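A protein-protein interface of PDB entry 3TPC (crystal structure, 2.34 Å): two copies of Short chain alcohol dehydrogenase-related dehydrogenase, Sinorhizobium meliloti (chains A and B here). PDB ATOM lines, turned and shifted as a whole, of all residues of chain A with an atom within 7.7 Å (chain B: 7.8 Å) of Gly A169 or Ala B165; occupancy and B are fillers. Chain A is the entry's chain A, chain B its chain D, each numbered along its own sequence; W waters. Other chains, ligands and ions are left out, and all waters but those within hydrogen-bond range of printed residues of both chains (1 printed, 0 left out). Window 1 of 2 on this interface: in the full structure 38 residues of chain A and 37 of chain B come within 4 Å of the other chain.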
ATOM      1  N   VAL A 113     -36.187  -9.035  -2.932  1.00  0.00           N
ATOM      2  CA  VAL A 113     -35.238  -8.547  -1.954  1.00  0.00           C
ATOM      3  C   VAL A 113     -35.842  -7.605  -0.882  1.00  0.00           C
ATOM      4  O   VAL A 113     -35.524  -7.721   0.314  1.00  0.00           O
ATOM      5  CB  VAL A 113     -34.068  -7.842  -2.654  1.00  0.00           C
ATOM      6  CG1 VAL A 113     -33.108  -7.360  -1.623  1.00  0.00           C
ATOM      7  CG2 VAL A 113     -33.358  -8.805  -3.580  1.00  0.00           C
ATOM      8  N   ASN A 116     -38.347  -9.963   1.257  1.00  0.00           N
ATOM      9  CA  ASN A 116     -37.681 -11.045   1.955  1.00  0.00           C
ATOM     10  C   ASN A 116     -36.553 -10.620   2.896  1.00  0.00           C
ATOM     11  O   ASN A 116     -36.469 -11.112   3.995  1.00  0.00           O
ATOM     12  CB  ASN A 116     -37.195 -12.075   0.967  1.00  0.00           C
ATOM     13  CG  ASN A 116     -38.339 -12.875   0.354  1.00  0.00           C
ATOM     14  OD1 ASN A 116     -39.298 -13.234   1.032  1.00  0.00           O
ATOM     15  ND2 ASN A 116     -38.247 -13.141  -0.952  1.00  0.00           N
ATOM     16  N   LEU A 117     -35.715  -9.696   2.467  1.00  0.00           N
ATOM     17  CA  LEU A 117     -34.521  -9.376   3.199  1.00  0.00           C
ATOM     18  C   LEU A 117     -34.625  -8.091   4.008  1.00  0.00           C
ATOM     19  O   LEU A 117     -34.307  -8.077   5.213  1.00  0.00           O
ATOM     20  CB  LEU A 117     -33.324  -9.303   2.256  1.00  0.00           C
ATOM     21  CG  LEU A 117     -31.984  -8.879   2.837  1.00  0.00           C
ATOM     22  CD1 LEU A 117     -31.572  -9.772   4.026  1.00  0.00           C
ATOM     23  CD2 LEU A 117     -31.019  -8.983   1.760  1.00  0.00           C
ATOM     24  N   THR A 120     -37.402  -8.341   6.852  1.00  0.00           N
ATOM     25  CA  THR A 120     -36.978  -9.059   8.043  1.00  0.00           C
ATOM     26  C   THR A 120     -35.892  -8.279   8.777  1.00  0.00           C
ATOM     27  O   THR A 120     -35.887  -8.259   9.994  1.00  0.00           O
ATOM     28  CB  THR A 120     -36.569 -10.489   7.790  1.00  0.00           C
ATOM     29  OG1 THR A 120     -35.408 -10.465   7.022  1.00  0.00           O
ATOM     30  CG2 THR A 120     -37.557 -11.224   6.978  1.00  0.00           C
ATOM     31  N   PHE A 121     -35.030  -7.552   8.071  1.00  0.00           N
ATOM     32  CA  PHE A 121     -34.067  -6.733   8.827  1.00  0.00           C
ATOM     33  C   PHE A 121     -34.731  -5.582   9.614  1.00  0.00           C
ATOM     34  O   PHE A 121     -34.384  -5.259  10.757  1.00  0.00           O
ATOM     35  CB  PHE A 121     -32.909  -6.247   7.945  1.00  0.00           C
ATOM     36  CG  PHE A 121     -31.905  -5.409   8.691  1.00  0.00           C
ATOM     37  CD1 PHE A 121     -30.907  -6.011   9.465  1.00  0.00           C
ATOM     38  CD2 PHE A 121     -31.992  -4.022   8.665  1.00  0.00           C
ATOM     39  CE1 PHE A 121     -29.996  -5.229  10.174  1.00  0.00           C
ATOM     40  CE2 PHE A 121     -31.079  -3.237   9.353  1.00  0.00           C
ATOM     41  CZ  PHE A 121     -30.096  -3.835  10.122  1.00  0.00           C
ATOM     42  N   ALA A 149     -35.349 -18.428   5.909  1.00  0.00           N
ATOM     43  CA  ALA A 149     -34.611 -18.345   4.658  1.00  0.00           C
ATOM     44  C   ALA A 149     -35.362 -19.326   3.779  1.00  0.00           C
ATOM     45  O   ALA A 149     -36.581 -19.349   3.792  1.00  0.00           O
ATOM     46  CB  ALA A 149     -33.168 -18.792   4.840  1.00  0.00           C
ATOM     47  N   ALA A 153     -31.430 -20.778  -0.847  1.00  0.00           N
ATOM     48  CA  ALA A 153     -30.294 -19.969  -0.490  1.00  0.00           C
ATOM     49  C   ALA A 153     -29.007 -20.715  -0.831  1.00  0.00           C
ATOM     50  O   ALA A 153     -28.015 -20.071  -1.140  1.00  0.00           O
ATOM     51  CB  ALA A 153     -30.326 -19.634   0.996  1.00  0.00           C
ATOM     52  N   ALA A 162     -33.883 -14.362  -7.887  1.00  0.00           N
ATOM     53  CA  ALA A 162     -34.315 -13.314  -6.934  1.00  0.00           C
ATOM     54  C   ALA A 162     -34.535 -13.919  -5.532  1.00  0.00           C
ATOM     55  O   ALA A 162     -34.020 -13.455  -4.545  1.00  0.00           O
ATOM     56  CB  ALA A 162     -35.608 -12.617  -7.421  1.00  0.00           C
ATOM     57  N   TYR A 163     -35.279 -15.003  -5.521  1.00  0.00           N
ATOM     58  CA  TYR A 163     -35.637 -15.717  -4.350  1.00  0.00           C
ATOM     59  C   TYR A 163     -34.388 -16.210  -3.637  1.00  0.00           C
ATOM     60  O   TYR A 163     -34.196 -15.868  -2.478  1.00  0.00           O
ATOM     61  CB  TYR A 163     -36.554 -16.889  -4.712  1.00  0.00           C
ATOM     62  CG  TYR A 163     -37.117 -17.553  -3.480  1.00  0.00           C
ATOM     63  CD1 TYR A 163     -37.825 -16.821  -2.558  1.00  0.00           C
ATOM     64  CD2 TYR A 163     -36.965 -18.910  -3.248  1.00  0.00           C
ATOM     65  CE1 TYR A 163     -38.351 -17.404  -1.461  1.00  0.00           C
ATOM     66  CE2 TYR A 163     -37.479 -19.485  -2.143  1.00  0.00           C
ATOM     67  CZ  TYR A 163     -38.173 -18.730  -1.250  1.00  0.00           C
ATOM     68  OH  TYR A 163     -38.733 -19.281  -0.120  1.00  0.00           O
ATOM     69  N   ALA A 164     -33.545 -16.976  -4.335  1.00  0.00           N
ATOM     70  CA  ALA A 164     -32.284 -17.455  -3.755  1.00  0.00           C
ATOM     71  C   ALA A 164     -31.389 -16.295  -3.216  1.00  0.00           C
ATOM     72  O   ALA A 164     -30.810 -16.423  -2.153  1.00  0.00           O
ATOM     73  CB  ALA A 164     -31.493 -18.269  -4.813  1.00  0.00           C
ATOM     74  N   ALA A 165     -31.236 -15.201  -3.977  1.00  0.00           N
ATOM     75  CA  ALA A 165     -30.407 -14.080  -3.514  1.00  0.00           C
ATOM     76  C   ALA A 165     -30.968 -13.483  -2.190  1.00  0.00           C
ATOM     77  O   ALA A 165     -30.242 -13.166  -1.251  1.00  0.00           O
ATOM     78  CB  ALA A 165     -30.306 -12.979  -4.625  1.00  0.00           C
ATOM     79  N   SER A 166     -32.275 -13.390  -2.163  1.00  0.00           N
ATOM     80  CA  SER A 166     -33.075 -12.870  -1.081  1.00  0.00           C
ATOM     81  C   SER A 166     -32.877 -13.627   0.229  1.00  0.00           C
ATOM     82  O   SER A 166     -32.628 -13.047   1.281  1.00  0.00           O
ATOM     83  CB  SER A 166     -34.531 -13.175  -1.473  1.00  0.00           C
ATOM     84  OG  SER A 166     -35.223 -12.008  -1.444  1.00  0.00           O
ATOM     85  N   LYS A 167     -33.046 -14.938   0.148  1.00  0.00           N
ATOM     86  CA  LYS A 167     -32.976 -15.804   1.273  1.00  0.00           C
ATOM     87  C   LYS A 167     -31.521 -16.094   1.635  1.00  0.00           C
ATOM     88  O   LYS A 167     -31.220 -16.455   2.771  1.00  0.00           O
ATOM     89  CB  LYS A 167     -33.743 -17.089   0.949  1.00  0.00           C
ATOM     90  CG  LYS A 167     -35.174 -16.803   0.580  1.00  0.00           C
ATOM     91  CD  LYS A 167     -35.845 -15.926   1.617  1.00  0.00           C
ATOM     92  CE  LYS A 167     -37.301 -16.314   1.618  1.00  0.00           C
ATOM     93  NZ  LYS A 167     -38.045 -16.087   2.915  1.00  0.00           N
ATOM     94  N   GLY A 168     -30.636 -15.979   0.659  1.00  0.00           N
ATOM     95  CA  GLY A 168     -29.210 -16.065   0.909  1.00  0.00           C
ATOM     96  C   GLY A 168     -28.785 -14.873   1.754  1.00  0.00           C
ATOM     97  O   GLY A 168     -27.972 -15.048   2.643  1.00  0.00           O
ATOM     98  N   GLY A 169     -29.331 -13.682   1.506  1.00  0.00           N
ATOM     99  CA  GLY A 169     -29.091 -12.497   2.353  1.00  0.00           C
ATOM    100  C   GLY A 169     -29.598 -12.733   3.769  1.00  0.00           C
ATOM    101  O   GLY A 169     -28.900 -12.414   4.746  1.00  0.00           O
ATOM    102  N   VAL A 170     -30.791 -13.345   3.912  1.00  0.00           N
ATOM    103  CA  VAL A 170     -31.280 -13.689   5.252  1.00  0.00           C
ATOM    104  C   VAL A 170     -30.343 -14.699   5.975  1.00  0.00           C
ATOM    105  O   VAL A 170     -29.998 -14.535   7.192  1.00  0.00           O
ATOM    106  CB  VAL A 170     -32.733 -14.242   5.212  1.00  0.00           C
ATOM    107  CG1 VAL A 170     -33.199 -14.773   6.634  1.00  0.00           C
ATOM    108  CG2 VAL A 170     -33.744 -13.175   4.623  1.00  0.00           C
ATOM    109  N   ALA A 171     -30.016 -15.787   5.272  1.00  0.00           N
ATOM    110  CA  ALA A 171     -29.142 -16.786   5.831  1.00  0.00           C
ATOM    111  C   ALA A 171     -27.812 -16.147   6.295  1.00  0.00           C
ATOM    112  O   ALA A 171     -27.449 -16.358   7.405  1.00  0.00           O
ATOM    113  CB  ALA A 171     -28.881 -17.902   4.793  1.00  0.00           C
ATOM    114  N   ALA A 172     -27.107 -15.389   5.435  1.00  0.00           N
ATOM    115  CA  ALA A 172     -25.910 -14.559   5.797  1.00  0.00           C
ATOM    116  C   ALA A 172     -26.021 -13.609   7.004  1.00  0.00           C
ATOM    117  O   ALA A 172     -25.033 -13.341   7.744  1.00  0.00           O
ATOM    118  CB  ALA A 172     -25.512 -13.701   4.574  1.00  0.00           C
ATOM    119  N   LEU A 173     -27.212 -13.075   7.200  1.00  0.00           N
ATOM    120  CA  LEU A 173     -27.433 -12.086   8.233  1.00  0.00           C
ATOM    121  C   LEU A 173     -27.424 -12.709   9.623  1.00  0.00           C
ATOM    122  O   LEU A 173     -27.157 -12.055  10.596  1.00  0.00           O
ATOM    123  CB  LEU A 173     -28.777 -11.422   7.983  1.00  0.00           C
ATOM    124  CG  LEU A 173     -29.202 -10.224   8.860  1.00  0.00           C
ATOM    125  CD1 LEU A 173     -28.230  -9.036   8.587  1.00  0.00           C
ATOM    126  CD2 LEU A 173     -30.589  -9.843   8.466  1.00  0.00           C
ATOM    127  N   THR A 174     -27.777 -13.977   9.717  1.00  0.00           N
ATOM    128  CA  THR A 174     -27.954 -14.588  11.004  1.00  0.00           C
ATOM    129  C   THR A 174     -26.777 -14.435  12.009  1.00  0.00           C
ATOM    130  O   THR A 174     -26.984 -14.112  13.164  1.00  0.00           O
ATOM    131  CB  THR A 174     -28.142 -16.089  10.843  1.00  0.00           C
ATOM    132  OG1 THR A 174     -29.043 -16.310   9.785  1.00  0.00           O
ATOM    133  CG2 THR A 174     -28.689 -16.640  12.067  1.00  0.00           C
ATOM    134  N   PRO A 176     -23.851 -12.366  11.968  1.00  0.00           N
ATOM    135  CA  PRO A 176     -23.460 -11.067  12.541  1.00  0.00           C
ATOM    136  C   PRO A 176     -24.542 -10.500  13.458  1.00  0.00           C
ATOM    137  O   PRO A 176     -24.230  -9.824  14.438  1.00  0.00           O
ATOM    138  CB  PRO A 176     -23.266 -10.186  11.319  1.00  0.00           C
ATOM    139  CG  PRO A 176     -23.784 -11.067  10.107  1.00  0.00           C
ATOM    140  CD  PRO A 176     -23.555 -12.422  10.523  1.00  0.00           C
ATOM    141  N   THR A 190     -31.899 -19.093  12.063  1.00  0.00           N
ATOM    142  CA  THR A 190     -32.630 -18.998  10.794  1.00  0.00           C
ATOM    143  C   THR A 190     -32.959 -20.403  10.385  1.00  0.00           C
ATOM    144  O   THR A 190     -32.115 -21.281  10.539  1.00  0.00           O
ATOM    145  CB  THR A 190     -31.738 -18.351   9.659  1.00  0.00           C
ATOM    146  OG1 THR A 190     -31.674 -16.948   9.839  1.00  0.00           O
ATOM    147  CG2 THR A 190     -32.291 -18.596   8.263  1.00  0.00           C
ATOM    148  N   PHE B 109     -29.316   0.550   5.177  1.00  0.00           N
ATOM    149  CA  PHE B 109     -29.267  -0.893   4.938  1.00  0.00           C
ATOM    150  C   PHE B 109     -29.717  -1.259   3.497  1.00  0.00           C
ATOM    151  O   PHE B 109     -28.995  -1.962   2.757  1.00  0.00           O
ATOM    152  CB  PHE B 109     -30.123  -1.615   5.996  1.00  0.00           C
ATOM    153  CG  PHE B 109     -30.164  -3.070   5.821  1.00  0.00           C
ATOM    154  CD1 PHE B 109     -29.302  -3.885   6.533  1.00  0.00           C
ATOM    155  CD2 PHE B 109     -31.065  -3.653   4.904  1.00  0.00           C
ATOM    156  CE1 PHE B 109     -29.302  -5.270   6.333  1.00  0.00           C
ATOM    157  CE2 PHE B 109     -31.097  -5.039   4.712  1.00  0.00           C
ATOM    158  CZ  PHE B 109     -30.204  -5.836   5.405  1.00  0.00           C
ATOM    159  N   THR B 112     -27.035  -0.168   0.891  1.00  0.00           N
ATOM    160  CA  THR B 112     -25.950  -1.130   0.784  1.00  0.00           C
ATOM    161  C   THR B 112     -26.367  -2.380   0.039  1.00  0.00           C
ATOM    162  O   THR B 112     -25.586  -2.907  -0.758  1.00  0.00           O
ATOM    163  CB  THR B 112     -25.536  -1.546   2.183  1.00  0.00           C
ATOM    164  OG1 THR B 112     -25.025  -0.399   2.858  1.00  0.00           O
ATOM    165  CG2 THR B 112     -24.494  -2.665   2.157  1.00  0.00           C
ATOM    166  N   VAL B 113     -27.585  -2.861   0.303  1.00  0.00           N
ATOM    167  CA  VAL B 113     -28.168  -3.954  -0.481  1.00  0.00           C
ATOM    168  C   VAL B 113     -28.325  -3.533  -1.946  1.00  0.00           C
ATOM    169  O   VAL B 113     -28.014  -4.302  -2.844  1.00  0.00           O
ATOM    170  CB  VAL B 113     -29.531  -4.432   0.106  1.00  0.00           C
ATOM    171  CG1 VAL B 113     -30.176  -5.511  -0.761  1.00  0.00           C
ATOM    172  CG2 VAL B 113     -29.327  -5.002   1.464  1.00  0.00           C
ATOM    173  N   ASN B 116     -24.622  -3.243  -3.604  1.00  0.00           N
ATOM    174  CA  ASN B 116     -23.919  -4.521  -3.622  1.00  0.00           C
ATOM    175  C   ASN B 116     -24.706  -5.631  -4.342  1.00  0.00           C
ATOM    176  O   ASN B 116     -24.142  -6.341  -5.155  1.00  0.00           O
ATOM    177  CB  ASN B 116     -23.491  -4.919  -2.196  1.00  0.00           C
ATOM    178  CG  ASN B 116     -22.381  -4.004  -1.636  1.00  0.00           C
ATOM    179  OD1 ASN B 116     -21.548  -3.521  -2.366  1.00  0.00           O
ATOM    180  ND2 ASN B 116     -22.389  -3.773  -0.353  1.00  0.00           N
ATOM    181  N   LEU B 117     -26.010  -5.732  -4.094  1.00  0.00           N
ATOM    182  CA  LEU B 117     -26.803  -6.815  -4.643  1.00  0.00           C
ATOM    183  C   LEU B 117     -27.642  -6.432  -5.901  1.00  0.00           C
ATOM    184  O   LEU B 117     -27.517  -7.087  -6.938  1.00  0.00           O
ATOM    185  CB  LEU B 117     -27.661  -7.463  -3.540  1.00  0.00           C
ATOM    186  CG  LEU B 117     -28.705  -8.487  -4.006  1.00  0.00           C
ATOM    187  CD1 LEU B 117     -28.104  -9.624  -4.885  1.00  0.00           C
ATOM    188  CD2 LEU B 117     -29.388  -9.083  -2.808  1.00  0.00           C
ATOM    189  N   ALA B 152     -17.336 -11.778   4.508  1.00  0.00           N
ATOM    190  CA  ALA B 152     -18.375 -11.409   5.450  1.00  0.00           C
ATOM    191  C   ALA B 152     -19.676 -12.143   5.100  1.00  0.00           C
ATOM    192  O   ALA B 152     -20.548 -12.271   5.941  1.00  0.00           O
ATOM    193  CB  ALA B 152     -18.579  -9.942   5.419  1.00  0.00           C
ATOM    194  N   ALA B 153     -19.786 -12.681   3.889  1.00  0.00           N
ATOM    195  CA  ALA B 153     -20.983 -13.475   3.554  1.00  0.00           C
ATOM    196  C   ALA B 153     -21.117 -14.750   4.410  1.00  0.00           C
ATOM    197  O   ALA B 153     -22.189 -15.277   4.570  1.00  0.00           O
ATOM    198  CB  ALA B 153     -21.048 -13.798   2.043  1.00  0.00           C
ATOM    199  N   GLY B 156     -19.778 -13.037   8.913  1.00  0.00           N
ATOM    200  CA  GLY B 156     -20.175 -11.699   9.253  1.00  0.00           C
ATOM    201  C   GLY B 156     -19.801 -11.273  10.669  1.00  0.00           C
ATOM    202  O   GLY B 156     -20.187 -11.916  11.675  1.00  0.00           O
ATOM    203  N   GLN B 160     -21.448  -5.695  10.775  1.00  0.00           N
ATOM    204  CA  GLN B 160     -21.421  -5.922   9.340  1.00  0.00           C
ATOM    205  C   GLN B 160     -22.716  -6.436   8.739  1.00  0.00           C
ATOM    206  O   GLN B 160     -22.699  -6.897   7.609  1.00  0.00           O
ATOM    207  CB  GLN B 160     -20.311  -6.883   8.962  1.00  0.00           C
ATOM    208  CG  GLN B 160     -18.911  -6.331   9.072  1.00  0.00           C
ATOM    209  CD  GLN B 160     -17.904  -7.197   8.348  1.00  0.00           C
ATOM    210  OE1 GLN B 160     -17.764  -8.413   8.622  1.00  0.00           O
ATOM    211  NE2 GLN B 160     -17.176  -6.575   7.415  1.00  0.00           N
ATOM    212  N   ALA B 161     -23.812  -6.354   9.480  1.00  0.00           N
ATOM    213  CA  ALA B 161     -25.074  -6.932   9.041  1.00  0.00           C
ATOM    214  C   ALA B 161     -25.467  -6.687   7.567  1.00  0.00           C
ATOM    215  O   ALA B 161     -25.865  -7.622   6.845  1.00  0.00           O
ATOM    216  CB  ALA B 161     -26.221  -6.471   9.949  1.00  0.00           C
ATOM    217  N   ALA B 162     -25.396  -5.430   7.154  1.00  0.00           N
ATOM    218  CA  ALA B 162     -25.887  -4.981   5.851  1.00  0.00           C
ATOM    219  C   ALA B 162     -24.934  -5.473   4.778  1.00  0.00           C
ATOM    220  O   ALA B 162     -25.351  -5.937   3.704  1.00  0.00           O
ATOM    221  CB  ALA B 162     -26.014  -3.430   5.818  1.00  0.00           C
ATOM    222  N   TYR B 163     -23.650  -5.416   5.109  1.00  0.00           N
ATOM    223  CA  TYR B 163     -22.586  -5.842   4.217  1.00  0.00           C
ATOM    224  C   TYR B 163     -22.651  -7.367   4.006  1.00  0.00           C
ATOM    225  O   TYR B 163     -22.701  -7.868   2.890  1.00  0.00           O
ATOM    226  CB  TYR B 163     -21.252  -5.460   4.827  1.00  0.00           C
ATOM    227  CG  TYR B 163     -20.090  -5.713   3.916  1.00  0.00           C
ATOM    228  CD1 TYR B 163     -20.115  -5.286   2.596  1.00  0.00           C
ATOM    229  CD2 TYR B 163     -18.964  -6.375   4.365  1.00  0.00           C
ATOM    230  CE1 TYR B 163     -19.049  -5.502   1.752  1.00  0.00           C
ATOM    231  CE2 TYR B 163     -17.878  -6.613   3.522  1.00  0.00           C
ATOM    232  CZ  TYR B 163     -17.936  -6.165   2.218  1.00  0.00           C
ATOM    233  OH  TYR B 163     -16.855  -6.341   1.384  1.00  0.00           O
ATOM    234  N   ALA B 164     -22.673  -8.088   5.102  1.00  0.00           N
ATOM    235  CA  ALA B 164     -22.819  -9.509   5.089  1.00  0.00           C
ATOM    236  C   ALA B 164     -24.083 -10.010   4.316  1.00  0.00           C
ATOM    237  O   ALA B 164     -23.996 -10.906   3.466  1.00  0.00           O
ATOM    238  CB  ALA B 164     -22.791 -10.017   6.533  1.00  0.00           C
ATOM    239  N   ALA B 165     -25.227  -9.412   4.592  1.00  0.00           N
ATOM    240  CA  ALA B 165     -26.461  -9.861   3.940  1.00  0.00           C
ATOM    241  C   ALA B 165     -26.376  -9.638   2.439  1.00  0.00           C
ATOM    242  O   ALA B 165     -26.680 -10.550   1.648  1.00  0.00           O
ATOM    243  CB  ALA B 165     -27.729  -9.151   4.533  1.00  0.00           C
ATOM    244  N   SER B 166     -25.998  -8.415   2.078  1.00  0.00           N
ATOM    245  CA  SER B 166     -25.668  -7.991   0.712  1.00  0.00           C
ATOM    246  C   SER B 166     -24.884  -9.046  -0.069  1.00  0.00           C
ATOM    247  O   SER B 166     -25.212  -9.414  -1.189  1.00  0.00           O
ATOM    248  CB  SER B 166     -24.647  -6.858   0.826  1.00  0.00           C
ATOM    249  OG  SER B 166     -25.261  -5.657   0.655  1.00  0.00           O
ATOM    250  N   LYS B 167     -23.742  -9.414   0.519  1.00  0.00           N
ATOM    251  CA  LYS B 167     -22.756 -10.203  -0.159  1.00  0.00           C
ATOM    252  C   LYS B 167     -23.197 -11.642  -0.127  1.00  0.00           C
ATOM    253  O   LYS B 167     -22.875 -12.428  -1.053  1.00  0.00           O
ATOM    254  CB  LYS B 167     -21.420 -10.030   0.541  1.00  0.00           C
ATOM    255  CG  LYS B 167     -20.793  -8.614   0.385  1.00  0.00           C
ATOM    256  CD  LYS B 167     -20.683  -8.180  -1.063  1.00  0.00           C
ATOM    257  CE  LYS B 167     -19.637  -7.098  -1.289  1.00  0.00           C
ATOM    258  NZ  LYS B 167     -19.365  -6.997  -2.764  1.00  0.00           N
ATOM    259  N   GLY B 168     -23.911 -11.991   0.947  1.00  0.00           N
ATOM    260  CA  GLY B 168     -24.539 -13.305   1.088  1.00  0.00           C
ATOM    261  C   GLY B 168     -25.529 -13.486  -0.035  1.00  0.00           C
ATOM    262  O   GLY B 168     -25.591 -14.546  -0.601  1.00  0.00           O
ATOM    263  N   GLY B 169     -26.252 -12.408  -0.384  1.00  0.00           N
ATOM    264  CA  GLY B 169     -27.125 -12.351  -1.527  1.00  0.00           C
ATOM    265  C   GLY B 169     -26.373 -12.678  -2.789  1.00  0.00           C
ATOM    266  O   GLY B 169     -26.829 -13.527  -3.618  1.00  0.00           O
ATOM    267  N   VAL B 170     -25.206 -12.035  -2.945  1.00  0.00           N
ATOM    268  CA  VAL B 170     -24.406 -12.187  -4.164  1.00  0.00           C
ATOM    269  C   VAL B 170     -23.876 -13.597  -4.293  1.00  0.00           C
ATOM    270  O   VAL B 170     -23.930 -14.197  -5.370  1.00  0.00           O
ATOM    271  CB  VAL B 170     -23.233 -11.133  -4.209  1.00  0.00           C
ATOM    272  CG1 VAL B 170     -22.114 -11.500  -5.282  1.00  0.00           C
ATOM    273  CG2 VAL B 170     -23.786  -9.786  -4.496  1.00  0.00           C
ATOM    274  N   ALA B 171     -23.303 -14.099  -3.199  1.00  0.00           N
ATOM    275  CA  ALA B 171     -22.864 -15.494  -3.139  1.00  0.00           C
ATOM    276  C   ALA B 171     -24.027 -16.439  -3.513  1.00  0.00           C
ATOM    277  O   ALA B 171     -23.837 -17.334  -4.286  1.00  0.00           O
ATOM    278  CB  ALA B 171     -22.297 -15.847  -1.692  1.00  0.00           C
ATOM    279  N   ALA B 172     -25.211 -16.267  -2.931  1.00  0.00           N
ATOM    280  CA  ALA B 172     -26.298 -17.221  -3.185  1.00  0.00           C
ATOM    281  C   ALA B 172     -26.828 -17.159  -4.628  1.00  0.00           C
ATOM    282  O   ALA B 172     -27.462 -18.103  -5.125  1.00  0.00           O
ATOM    283  CB  ALA B 172     -27.450 -17.004  -2.181  1.00  0.00           C
ATOM    284  N   LEU B 173     -26.558 -16.041  -5.306  1.00  0.00           N
ATOM    285  CA  LEU B 173     -27.061 -15.843  -6.657  1.00  0.00           C
ATOM    286  C   LEU B 173     -26.280 -16.729  -7.637  1.00  0.00           C
ATOM    287  O   LEU B 173     -26.752 -17.109  -8.718  1.00  0.00           O
ATOM    288  CB  LEU B 173     -26.926 -14.362  -7.028  1.00  0.00           C
ATOM    289  CG  LEU B 173     -27.533 -13.741  -8.276  1.00  0.00           C
ATOM    290  CD1 LEU B 173     -29.062 -13.607  -8.189  1.00  0.00           C
ATOM    291  CD2 LEU B 173     -26.887 -12.367  -8.384  1.00  0.00           C
HETATM  292  O   HOH W   1     -28.247 -20.515  -4.175  1.00  0.00           O
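Water W1 lies within hydrogen-bond range of the backbone carbonyl oxygen of Ala B172 (2.7 Å) and the backbone carbonyl oxygen of Ala A153 (3.1 Å).
Printed residues of chain A that touch a printed residue of chain B: Val A113, Leu A117, Phe A121, Ala A153, Ala A164, Ala A165, Gly A168, Gly A169, Ala A172, Leu A173 and Pro A176.
Hydrophobic or aromatic side chains of chain A that line the printed part of chain B: Val A113, Leu A117, Phe A121, Ala A165, Ala A172, Leu A173 and Pro A176.
Among the printed residues, no Asp or Glu carboxylate lies within 4 Å of a Lys or Arg side-chain nitrogen of the other chain.
Val A113 touches its own counterpart, Val B113.
Ala A153 touches Ala B172, and with the chains exchanged Ala A172 touches Ala B153.
Ala A164 touches Ala B172, and with the chains exchanged Ala A172 touches Ala B164.
Gly A168 touches Ala B172, and with the chains exchanged Ala A172 touches Gly B168.
Of the 18 pairs that touch across the chains among the printed residues, 11 have their exchanged pair printed and touching as well.
Of chain B, only Ala B165 (3.2 Å) and Gly B169 (3.8 Å) come within 4 Å of Gly A169.
Of the printed residues of chain A, Ala B165 touches Leu A117 (3.9 Å) and Gly A169 (3.2 Å).
Gly A168 touches just these residues of chain B: Gly B168 and Ala B172.
Of the printed residues of chain A, Ala B161 touches Phe A121 (3.98 Å) and Leu A173 (3.3 Å).
Of the printed residues of chain A, Ala B172 touches Ala A153 (3.3 Å), Ala A164 (3.4 Å) and Gly A168 (3.7 Å).
Leu B117 touches none of the printed residues of chain A.
Among the printed residues, merely in contact across the chains: Val A113 with Val B113 (3.6 Å), Leu A117 with Ala B165 (3.9 Å), Phe A121 with Phe B109 (3.4 Å), Phe A121 with Ala B161 (3.98 Å), Ala A153 with Ala B172 (3.3 Å), Ala A164 with Ala B172 (3.4 Å), Ala A165 with Gly B169 (3.2 Å), Ala A165 with Leu B173 (3.8 Å), Gly A168 with Gly B168 (3.9 Å), Gly A168 with Ala B172 (3.7 Å), Gly A169 with Ala B165 (3.2 Å), Gly A169 with Gly B169 (3.8 Å), Ala A172 with Ala B153 (3.7 Å), Ala A172 with Ala B164 (3.4 Å), Ala A172 with Gly B168 (3.6 Å), Leu A173 with Ala B161 (3.3 Å), Pro A176 with Gly B156 (3.5 Å) and Pro A176 with Ala B164 (3.9 Å).
The backbone NH of Val A113 sits at hydrogen-bond distance from the side-chain hydroxyl of Ser A166 (3.5 Å).
The backbone carbonyl oxygen (O) of Leu A117 is in hydrogen-bond range of the side-chain hydroxyl (OG1) of Thr A120.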
